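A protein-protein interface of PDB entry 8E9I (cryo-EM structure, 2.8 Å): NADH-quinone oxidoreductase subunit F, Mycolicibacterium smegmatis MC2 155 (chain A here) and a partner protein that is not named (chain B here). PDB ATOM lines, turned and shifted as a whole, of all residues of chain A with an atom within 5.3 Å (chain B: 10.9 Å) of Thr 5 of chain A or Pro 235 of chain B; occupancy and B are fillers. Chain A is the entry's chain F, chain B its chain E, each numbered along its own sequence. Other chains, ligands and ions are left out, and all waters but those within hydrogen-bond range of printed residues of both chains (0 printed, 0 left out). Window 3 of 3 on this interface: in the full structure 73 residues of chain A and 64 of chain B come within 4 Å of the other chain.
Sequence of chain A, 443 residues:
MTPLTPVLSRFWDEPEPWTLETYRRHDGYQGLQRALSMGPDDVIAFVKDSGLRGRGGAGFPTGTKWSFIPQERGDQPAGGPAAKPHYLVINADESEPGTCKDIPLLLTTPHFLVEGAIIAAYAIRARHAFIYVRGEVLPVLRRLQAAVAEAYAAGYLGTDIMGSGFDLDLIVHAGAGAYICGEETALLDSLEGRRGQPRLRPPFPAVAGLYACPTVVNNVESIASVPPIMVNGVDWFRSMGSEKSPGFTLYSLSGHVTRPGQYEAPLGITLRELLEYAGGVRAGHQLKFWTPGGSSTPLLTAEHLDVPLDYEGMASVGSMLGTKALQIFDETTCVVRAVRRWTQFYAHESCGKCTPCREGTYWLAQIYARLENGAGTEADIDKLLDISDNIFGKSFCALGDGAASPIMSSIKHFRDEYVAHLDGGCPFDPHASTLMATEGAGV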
ATOM      1  N   PRO A   3     -22.434  -6.655   9.061  1.00  0.00           N
ATOM      2  CA  PRO A   3     -21.338  -6.650   8.089  1.00  0.00           C
ATOM      3  C   PRO A   3     -20.139  -5.847   8.560  1.00  0.00           C
ATOM      4  O   PRO A   3     -20.286  -4.926   9.367  1.00  0.00           O
ATOM      5  CB  PRO A   3     -21.987  -6.003   6.864  1.00  0.00           C
ATOM      6  CG  PRO A   3     -22.910  -4.991   7.472  1.00  0.00           C
ATOM      7  CD  PRO A   3     -23.404  -5.583   8.784  1.00  0.00           C
ATOM      8  N   LEU A   4     -18.952  -6.175   8.063  1.00  0.00           N
ATOM      9  CA  LEU A   4     -17.814  -5.303   8.281  1.00  0.00           C
ATOM     10  C   LEU A   4     -18.127  -3.918   7.726  1.00  0.00           C
ATOM     11  O   LEU A   4     -19.019  -3.739   6.894  1.00  0.00           O
ATOM     12  CB  LEU A   4     -16.562  -5.874   7.621  1.00  0.00           C
ATOM     13  CG  LEU A   4     -15.843  -6.954   8.427  1.00  0.00           C
ATOM     14  CD1 LEU A   4     -16.661  -8.235   8.451  1.00  0.00           C
ATOM     15  CD2 LEU A   4     -14.468  -7.214   7.853  1.00  0.00           C
ATOM     16  N   THR A   5     -17.388  -2.926   8.201  1.00  0.00           N
ATOM     17  CA  THR A   5     -17.692  -1.555   7.823  1.00  0.00           C
ATOM     18  C   THR A   5     -16.421  -0.719   7.764  1.00  0.00           C
ATOM     19  O   THR A   5     -16.214   0.160   8.609  1.00  0.00           O
ATOM     20  CB  THR A   5     -18.685  -0.954   8.815  1.00  0.00           C
ATOM     21  OG1 THR A   5     -19.792  -1.848   8.968  1.00  0.00           O
ATOM     22  CG2 THR A   5     -19.196   0.378   8.313  1.00  0.00           C
ATOM     23  N   PRO A   6     -15.553  -0.958   6.785  1.00  0.00           N
ATOM     24  CA  PRO A   6     -14.308  -0.186   6.700  1.00  0.00           C
ATOM     25  C   PRO A   6     -14.570   1.312   6.701  1.00  0.00           C
ATOM     26  O   PRO A   6     -15.209   1.852   5.795  1.00  0.00           O
ATOM     27  CB  PRO A   6     -13.692  -0.660   5.381  1.00  0.00           C
ATOM     28  CG  PRO A   6     -14.237  -2.028   5.194  1.00  0.00           C
ATOM     29  CD  PRO A   6     -15.632  -1.988   5.738  1.00  0.00           C
ATOM     30  N   VAL A   7     -14.074   1.976   7.743  1.00  0.00           N
ATOM     31  CA  VAL A   7     -14.180   3.421   7.894  1.00  0.00           C
ATOM     32  C   VAL A   7     -12.789   3.993   8.119  1.00  0.00           C
ATOM     33  O   VAL A   7     -12.327   4.847   7.357  1.00  0.00           O
ATOM     34  CB  VAL A   7     -15.126   3.787   9.048  1.00  0.00           C
ATOM     35  CG1 VAL A   7     -14.957   5.242   9.438  1.00  0.00           C
ATOM     36  CG2 VAL A   7     -16.556   3.508   8.643  1.00  0.00           C
ATOM     37  N   TRP A 236     -25.105   9.516  10.158  1.00  0.00           N
ATOM     38  CA  TRP A 236     -24.352   8.399   9.601  1.00  0.00           C
ATOM     39  C   TRP A 236     -23.781   7.525  10.708  1.00  0.00           C
ATOM     40  O   TRP A 236     -23.869   6.294  10.655  1.00  0.00           O
ATOM     41  CB  TRP A 236     -23.239   8.917   8.694  1.00  0.00           C
ATOM     42  CG  TRP A 236     -22.262   7.867   8.297  1.00  0.00           C
ATOM     43  CD1 TRP A 236     -22.407   6.956   7.301  1.00  0.00           C
ATOM     44  CD2 TRP A 236     -20.971   7.633   8.866  1.00  0.00           C
ATOM     45  NE1 TRP A 236     -21.297   6.157   7.218  1.00  0.00           N
ATOM     46  CE2 TRP A 236     -20.397   6.554   8.170  1.00  0.00           C
ATOM     47  CE3 TRP A 236     -20.247   8.228   9.901  1.00  0.00           C
ATOM     48  CZ2 TRP A 236     -19.137   6.058   8.474  1.00  0.00           C
ATOM     49  CZ3 TRP A 236     -18.997   7.736  10.198  1.00  0.00           C
ATOM     50  CH2 TRP A 236     -18.454   6.661   9.490  1.00  0.00           C
ATOM     51  N   SER A 239     -26.491   5.338  12.527  1.00  0.00           N
ATOM     52  CA  SER A 239     -27.031   4.205  11.792  1.00  0.00           C
ATOM     53  C   SER A 239     -26.374   2.896  12.203  1.00  0.00           C
ATOM     54  O   SER A 239     -27.015   1.843  12.131  1.00  0.00           O
ATOM     55  CB  SER A 239     -26.843   4.417  10.292  1.00  0.00           C
ATOM     56  OG  SER A 239     -25.521   4.088   9.902  1.00  0.00           O
ATOM     57  N   MET A 240     -25.122   2.942  12.632  1.00  0.00           N
ATOM     58  CA  MET A 240     -24.403   1.754  13.054  1.00  0.00           C
ATOM     59  C   MET A 240     -24.639   1.488  14.534  1.00  0.00           C
ATOM     60  O   MET A 240     -25.070   2.368  15.283  1.00  0.00           O
ATOM     61  CB  MET A 240     -22.911   1.926  12.778  1.00  0.00           C
ATOM     62  CG  MET A 240     -22.579   1.996  11.302  1.00  0.00           C
ATOM     63  SD  MET A 240     -20.817   2.141  10.991  1.00  0.00           S
ATOM     64  CE  MET A 240     -20.553   3.846  11.462  1.00  0.00           C
ATOM     65  N   PHE A 248     -18.972   2.490  15.108  1.00  0.00           N
ATOM     66  CA  PHE A 248     -18.113   1.453  14.567  1.00  0.00           C
ATOM     67  C   PHE A 248     -16.897   1.308  15.467  1.00  0.00           C
ATOM     68  O   PHE A 248     -16.515   2.237  16.180  1.00  0.00           O
ATOM     69  CB  PHE A 248     -17.667   1.794  13.148  1.00  0.00           C
ATOM     70  CG  PHE A 248     -16.866   3.057  13.060  1.00  0.00           C
ATOM     71  CD1 PHE A 248     -15.485   3.017  13.069  1.00  0.00           C
ATOM     72  CD2 PHE A 248     -17.493   4.284  12.992  1.00  0.00           C
ATOM     73  CE1 PHE A 248     -14.747   4.176  12.993  1.00  0.00           C
ATOM     74  CE2 PHE A 248     -16.761   5.445  12.919  1.00  0.00           C
ATOM     75  CZ  PHE A 248     -15.387   5.393  12.920  1.00  0.00           C
ATOM     76  N   GLU A 264     -13.068  -3.762  11.069  1.00  0.00           N
ATOM     77  CA  GLU A 264     -13.827  -2.579  11.452  1.00  0.00           C
ATOM     78  C   GLU A 264     -15.301  -2.883  11.241  1.00  0.00           C
ATOM     79  O   GLU A 264     -15.755  -2.992  10.098  1.00  0.00           O
ATOM     80  CB  GLU A 264     -13.401  -1.360  10.637  1.00  0.00           C
ATOM     81  N   ALA A 265     -16.044  -3.014  12.332  1.00  0.00           N
ATOM     82  CA  ALA A 265     -17.421  -3.472  12.247  1.00  0.00           C
ATOM     83  C   ALA A 265     -18.284  -2.599  13.139  1.00  0.00           C
ATOM     84  O   ALA A 265     -17.775  -1.947  14.057  1.00  0.00           O
ATOM     85  CB  ALA A 265     -17.551  -4.942  12.661  1.00  0.00           C
ATOM     86  N   PRO A 266     -19.593  -2.565  12.901  1.00  0.00           N
ATOM     87  CA  PRO A 266     -20.478  -1.821  13.800  1.00  0.00           C
ATOM     88  C   PRO A 266     -20.489  -2.449  15.182  1.00  0.00           C
ATOM     89  O   PRO A 266     -20.231  -3.642  15.349  1.00  0.00           O
ATOM     90  CB  PRO A 266     -21.851  -1.932  13.125  1.00  0.00           C
ATOM     91  CG  PRO A 266     -21.566  -2.362  11.726  1.00  0.00           C
ATOM     92  CD  PRO A 266     -20.345  -3.210  11.817  1.00  0.00           C
ATOM     93  N   LEU B 221      -4.773  -5.692   7.428  1.00  0.00           N
ATOM     94  CA  LEU B 221      -5.603  -5.593   6.238  1.00  0.00           C
ATOM     95  C   LEU B 221      -6.696  -6.647   6.180  1.00  0.00           C
ATOM     96  O   LEU B 221      -7.711  -6.415   5.520  1.00  0.00           O
ATOM     97  CB  LEU B 221      -4.730  -5.714   4.990  1.00  0.00           C
ATOM     98  CG  LEU B 221      -3.618  -4.674   4.871  1.00  0.00           C
ATOM     99  CD1 LEU B 221      -2.765  -4.954   3.650  1.00  0.00           C
ATOM    100  CD2 LEU B 221      -4.207  -3.283   4.805  1.00  0.00           C
ATOM    101  N   ALA B 222      -6.529  -7.774   6.876  1.00  0.00           N
ATOM    102  CA  ALA B 222      -7.470  -8.886   6.760  1.00  0.00           C
ATOM    103  C   ALA B 222      -8.918  -8.408   6.699  1.00  0.00           C
ATOM    104  O   ALA B 222      -9.698  -8.859   5.852  1.00  0.00           O
ATOM    105  CB  ALA B 222      -7.276  -9.848   7.930  1.00  0.00           C
ATOM    106  N   GLY B 223      -9.299  -7.494   7.590  1.00  0.00           N
ATOM    107  CA  GLY B 223     -10.681  -7.041   7.613  1.00  0.00           C
ATOM    108  C   GLY B 223     -11.077  -6.299   6.352  1.00  0.00           C
ATOM    109  O   GLY B 223     -12.146  -6.538   5.784  1.00  0.00           O
ATOM    110  N   LEU B 224     -10.228  -5.377   5.905  1.00  0.00           N
ATOM    111  CA  LEU B 224     -10.529  -4.628   4.691  1.00  0.00           C
ATOM    112  C   LEU B 224     -10.575  -5.554   3.485  1.00  0.00           C
ATOM    113  O   LEU B 224     -11.431  -5.411   2.604  1.00  0.00           O
ATOM    114  CB  LEU B 224      -9.488  -3.528   4.491  1.00  0.00           C
ATOM    115  CG  LEU B 224      -9.712  -2.614   3.291  1.00  0.00           C
ATOM    116  CD1 LEU B 224     -10.942  -1.754   3.503  1.00  0.00           C
ATOM    117  CD2 LEU B 224      -8.483  -1.756   3.037  1.00  0.00           C
ATOM    118  N   ARG B 225      -9.646  -6.506   3.424  1.00  0.00           N
ATOM    119  CA  ARG B 225      -9.631  -7.466   2.329  1.00  0.00           C
ATOM    120  C   ARG B 225     -10.919  -8.276   2.307  1.00  0.00           C
ATOM    121  O   ARG B 225     -11.516  -8.483   1.246  1.00  0.00           O
ATOM    122  CB  ARG B 225      -8.417  -8.387   2.452  1.00  0.00           C
ATOM    123  N   LEU B 226     -11.366  -8.739   3.475  1.00  0.00           N
ATOM    124  CA  LEU B 226     -12.607  -9.506   3.536  1.00  0.00           C
ATOM    125  C   LEU B 226     -13.799  -8.649   3.142  1.00  0.00           C
ATOM    126  O   LEU B 226     -14.710  -9.121   2.453  1.00  0.00           O
ATOM    127  CB  LEU B 226     -12.798 -10.084   4.936  1.00  0.00           C
ATOM    128  N   ALA B 227     -13.815  -7.386   3.567  1.00  0.00           N
ATOM    129  CA  ALA B 227     -14.899  -6.492   3.176  1.00  0.00           C
ATOM    130  C   ALA B 227     -14.939  -6.312   1.665  1.00  0.00           C
ATOM    131  O   ALA B 227     -16.005  -6.393   1.045  1.00  0.00           O
ATOM    132  CB  ALA B 227     -14.738  -5.141   3.869  1.00  0.00           C
ATOM    133  N   ARG B 228     -13.781  -6.069   1.052  1.00  0.00           N
ATOM    134  CA  ARG B 228     -13.738  -5.886  -0.395  1.00  0.00           C
ATOM    135  C   ARG B 228     -14.167  -7.159  -1.114  1.00  0.00           C
ATOM    136  O   ARG B 228     -14.935  -7.113  -2.080  1.00  0.00           O
ATOM    137  CB  ARG B 228     -12.334  -5.466  -0.828  1.00  0.00           C
ATOM    138  N   ARG B 230     -16.148  -9.374  -0.057  1.00  0.00           N
ATOM    139  CA  ARG B 230     -17.552  -9.656   0.200  1.00  0.00           C
ATOM    140  C   ARG B 230     -18.427  -8.416   0.058  1.00  0.00           C
ATOM    141  O   ARG B 230     -19.571  -8.423   0.526  1.00  0.00           O
ATOM    142  CB  ARG B 230     -17.729 -10.264   1.597  1.00  0.00           C
ATOM    143  N   GLY B 231     -17.923  -7.352  -0.563  1.00  0.00           N
ATOM    144  CA  GLY B 231     -18.761  -6.217  -0.900  1.00  0.00           C
ATOM    145  C   GLY B 231     -19.227  -5.381   0.268  1.00  0.00           C
ATOM    146  O   GLY B 231     -20.259  -4.716   0.165  1.00  0.00           O
ATOM    147  N   MET B 232     -18.498  -5.391   1.380  1.00  0.00           N
ATOM    148  CA  MET B 232     -18.838  -4.547   2.515  1.00  0.00           C
ATOM    149  C   MET B 232     -18.162  -3.186   2.386  1.00  0.00           C
ATOM    150  O   MET B 232     -17.134  -3.042   1.721  1.00  0.00           O
ATOM    151  CB  MET B 232     -18.416  -5.216   3.822  1.00  0.00           C
ATOM    152  N   THR B 233     -18.762  -2.178   3.017  1.00  0.00           N
ATOM    153  CA  THR B 233     -18.207  -0.833   3.006  1.00  0.00           C
ATOM    154  C   THR B 233     -18.971   0.029   3.999  1.00  0.00           C
ATOM    155  O   THR B 233     -19.998  -0.378   4.545  1.00  0.00           O
ATOM    156  CB  THR B 233     -18.267  -0.211   1.608  1.00  0.00           C
ATOM    157  OG1 THR B 233     -17.543   1.025   1.599  1.00  0.00           O
ATOM    158  CG2 THR B 233     -19.713   0.045   1.197  1.00  0.00           C
ATOM    159  N   ALA B 234     -18.450   1.234   4.233  1.00  0.00           N
ATOM    160  CA  ALA B 234     -19.138   2.229   5.047  1.00  0.00           C
ATOM    161  C   ALA B 234     -20.420   2.628   4.328  1.00  0.00           C
ATOM    162  O   ALA B 234     -20.390   2.871   3.116  1.00  0.00           O
ATOM    163  CB  ALA B 234     -18.249   3.447   5.292  1.00  0.00           C
ATOM    164  N   PRO B 235     -21.558   2.707   5.019  1.00  0.00           N
ATOM    165  CA  PRO B 235     -22.832   2.758   4.289  1.00  0.00           C
ATOM    166  C   PRO B 235     -22.977   3.948   3.352  1.00  0.00           C
ATOM    167  O   PRO B 235     -22.976   3.773   2.129  1.00  0.00           O
ATOM    168  CB  PRO B 235     -23.875   2.824   5.414  1.00  0.00           C
ATOM    169  CG  PRO B 235     -23.132   3.294   6.618  1.00  0.00           C
ATOM    170  CD  PRO B 235     -21.740   2.791   6.475  1.00  0.00           C
ATOM    171  N   THR B 236     -23.094   5.159   3.900  1.00  0.00           N
ATOM    172  CA  THR B 236     -23.144   6.380   3.099  1.00  0.00           C
ATOM    173  C   THR B 236     -23.415   7.564   4.020  1.00  0.00           C
ATOM    174  O   THR B 236     -24.103   7.400   5.033  1.00  0.00           O
ATOM    175  CB  THR B 236     -24.223   6.277   2.013  1.00  0.00           C
ATOM    176  OG1 THR B 236     -23.880   5.239   1.088  1.00  0.00           O
ATOM    177  CG2 THR B 236     -24.385   7.588   1.252  1.00  0.00           C
ATOM    178  N   PRO B 237     -22.955   8.777   3.687  1.00  0.00           N
ATOM    179  CA  PRO B 237     -23.362   9.960   4.450  1.00  0.00           C
ATOM    180  C   PRO B 237     -24.857  10.007   4.764  1.00  0.00           C
ATOM    181  O   PRO B 237     -25.649  10.326   3.878  1.00  0.00           O
ATOM    182  CB  PRO B 237     -22.969  11.104   3.522  1.00  0.00           C
ATOM    183  CG  PRO B 237     -21.738  10.598   2.840  1.00  0.00           C
ATOM    184  CD  PRO B 237     -21.834   9.086   2.783  1.00  0.00           C
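N of Met 232 of chain B sits at hydrogen-bond distance from O of Ala 227 of chain B, 2.7 Å away. O of Trp 236 of chain A lies within hydrogen-bond range of OG of Ser 239 of chain A, at 2.9 Å. OG1 of Thr 5 of chain A is in hydrogen-bond range of O of Pro 3 of chain A (3.1 Å). N of Thr 5 of chain A sits at hydrogen-bond distance from O of Glu 264 of chain A.
Among the printed residues, merely in contact across the chains: Trp 236 of chain A with Thr 236 of chain B (2.9 Å), Leu 4 of chain A with Gly 223 of chain B (3.2 Å), Pro 6 of chain A with Ala 227 of chain B (3.4 Å), Trp 236 of chain A with Pro 235 of chain B (3.5 Å), Leu 4 of chain A with Met 232 of chain B (3.5 Å), Pro 6 of chain A with Ala 234 of chain B (3.5 Å), Pro 6 of chain A with Leu 224 of chain B (3.5 Å), Thr 5 of chain A with Ala 234 of chain B (3.8 Å), Val 7 of chain A with Ala 234 of chain B (3.8 Å), Thr 5 of chain A with Thr 233 of chain B (3.9 Å), Pro 6 of chain A with Thr 233 of chain B (3.9 Å) and Thr 5 of chain A with Pro 235 of chain B (3.96 Å).
Pro 235 of chain B touches just these residues of chain A: Thr 5 and Trp 236. Leu 4 of chain A touches two residues of chain B. Of chain B, only Leu 224 (3.5 Å), Ala 227 (3.4 Å), Thr 233 (3.9 Å) and Ala 234 (3.5 Å) come within 4 Å of Pro 6 of chain A. No residue of chain B comes within 4 Å of Glu 264 of chain A. No residue of chain B comes within 4 Å of Ala 265 of chain A. No residue of chain B comes within 4 Å of Pro 266 of chain A. Printed residues of chain A within 4 Å of Ala 227 of chain B: Pro 6 (3.4 Å). Printed residues of chain A within 4 Å of Gly 223 of chain B: Leu 4 (3.2 Å). Of the printed residues of chain A, Thr 233 of chain B touches Thr 5 and Pro 6. Of the printed residues of chain A, Thr 236 of chain B touches Trp 236 (2.9 Å). The nearest printed residue of chain A that does not touch Met 232 of chain B is Pro 6 of chain A (4.4 Å).
Of the 16 printed residues of chain B, 8 touch a printed residue of chain A. Hydrophobic or aromatic side chains of chain B within 4 Å of the printed part of chain A: Leu 224, Ala 227, Met 232, Ala 234 and Pro 235. Of the 12 printed residues of chain A, 5 touch a printed residue of chain B. Hydrophobic or aromatic side chains of chain A within 4 Å of the printed part of chain B: Leu 4, Pro 6, Val 7 and Trp 236. Among the printed residues, 12 pairs touch across the chains.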
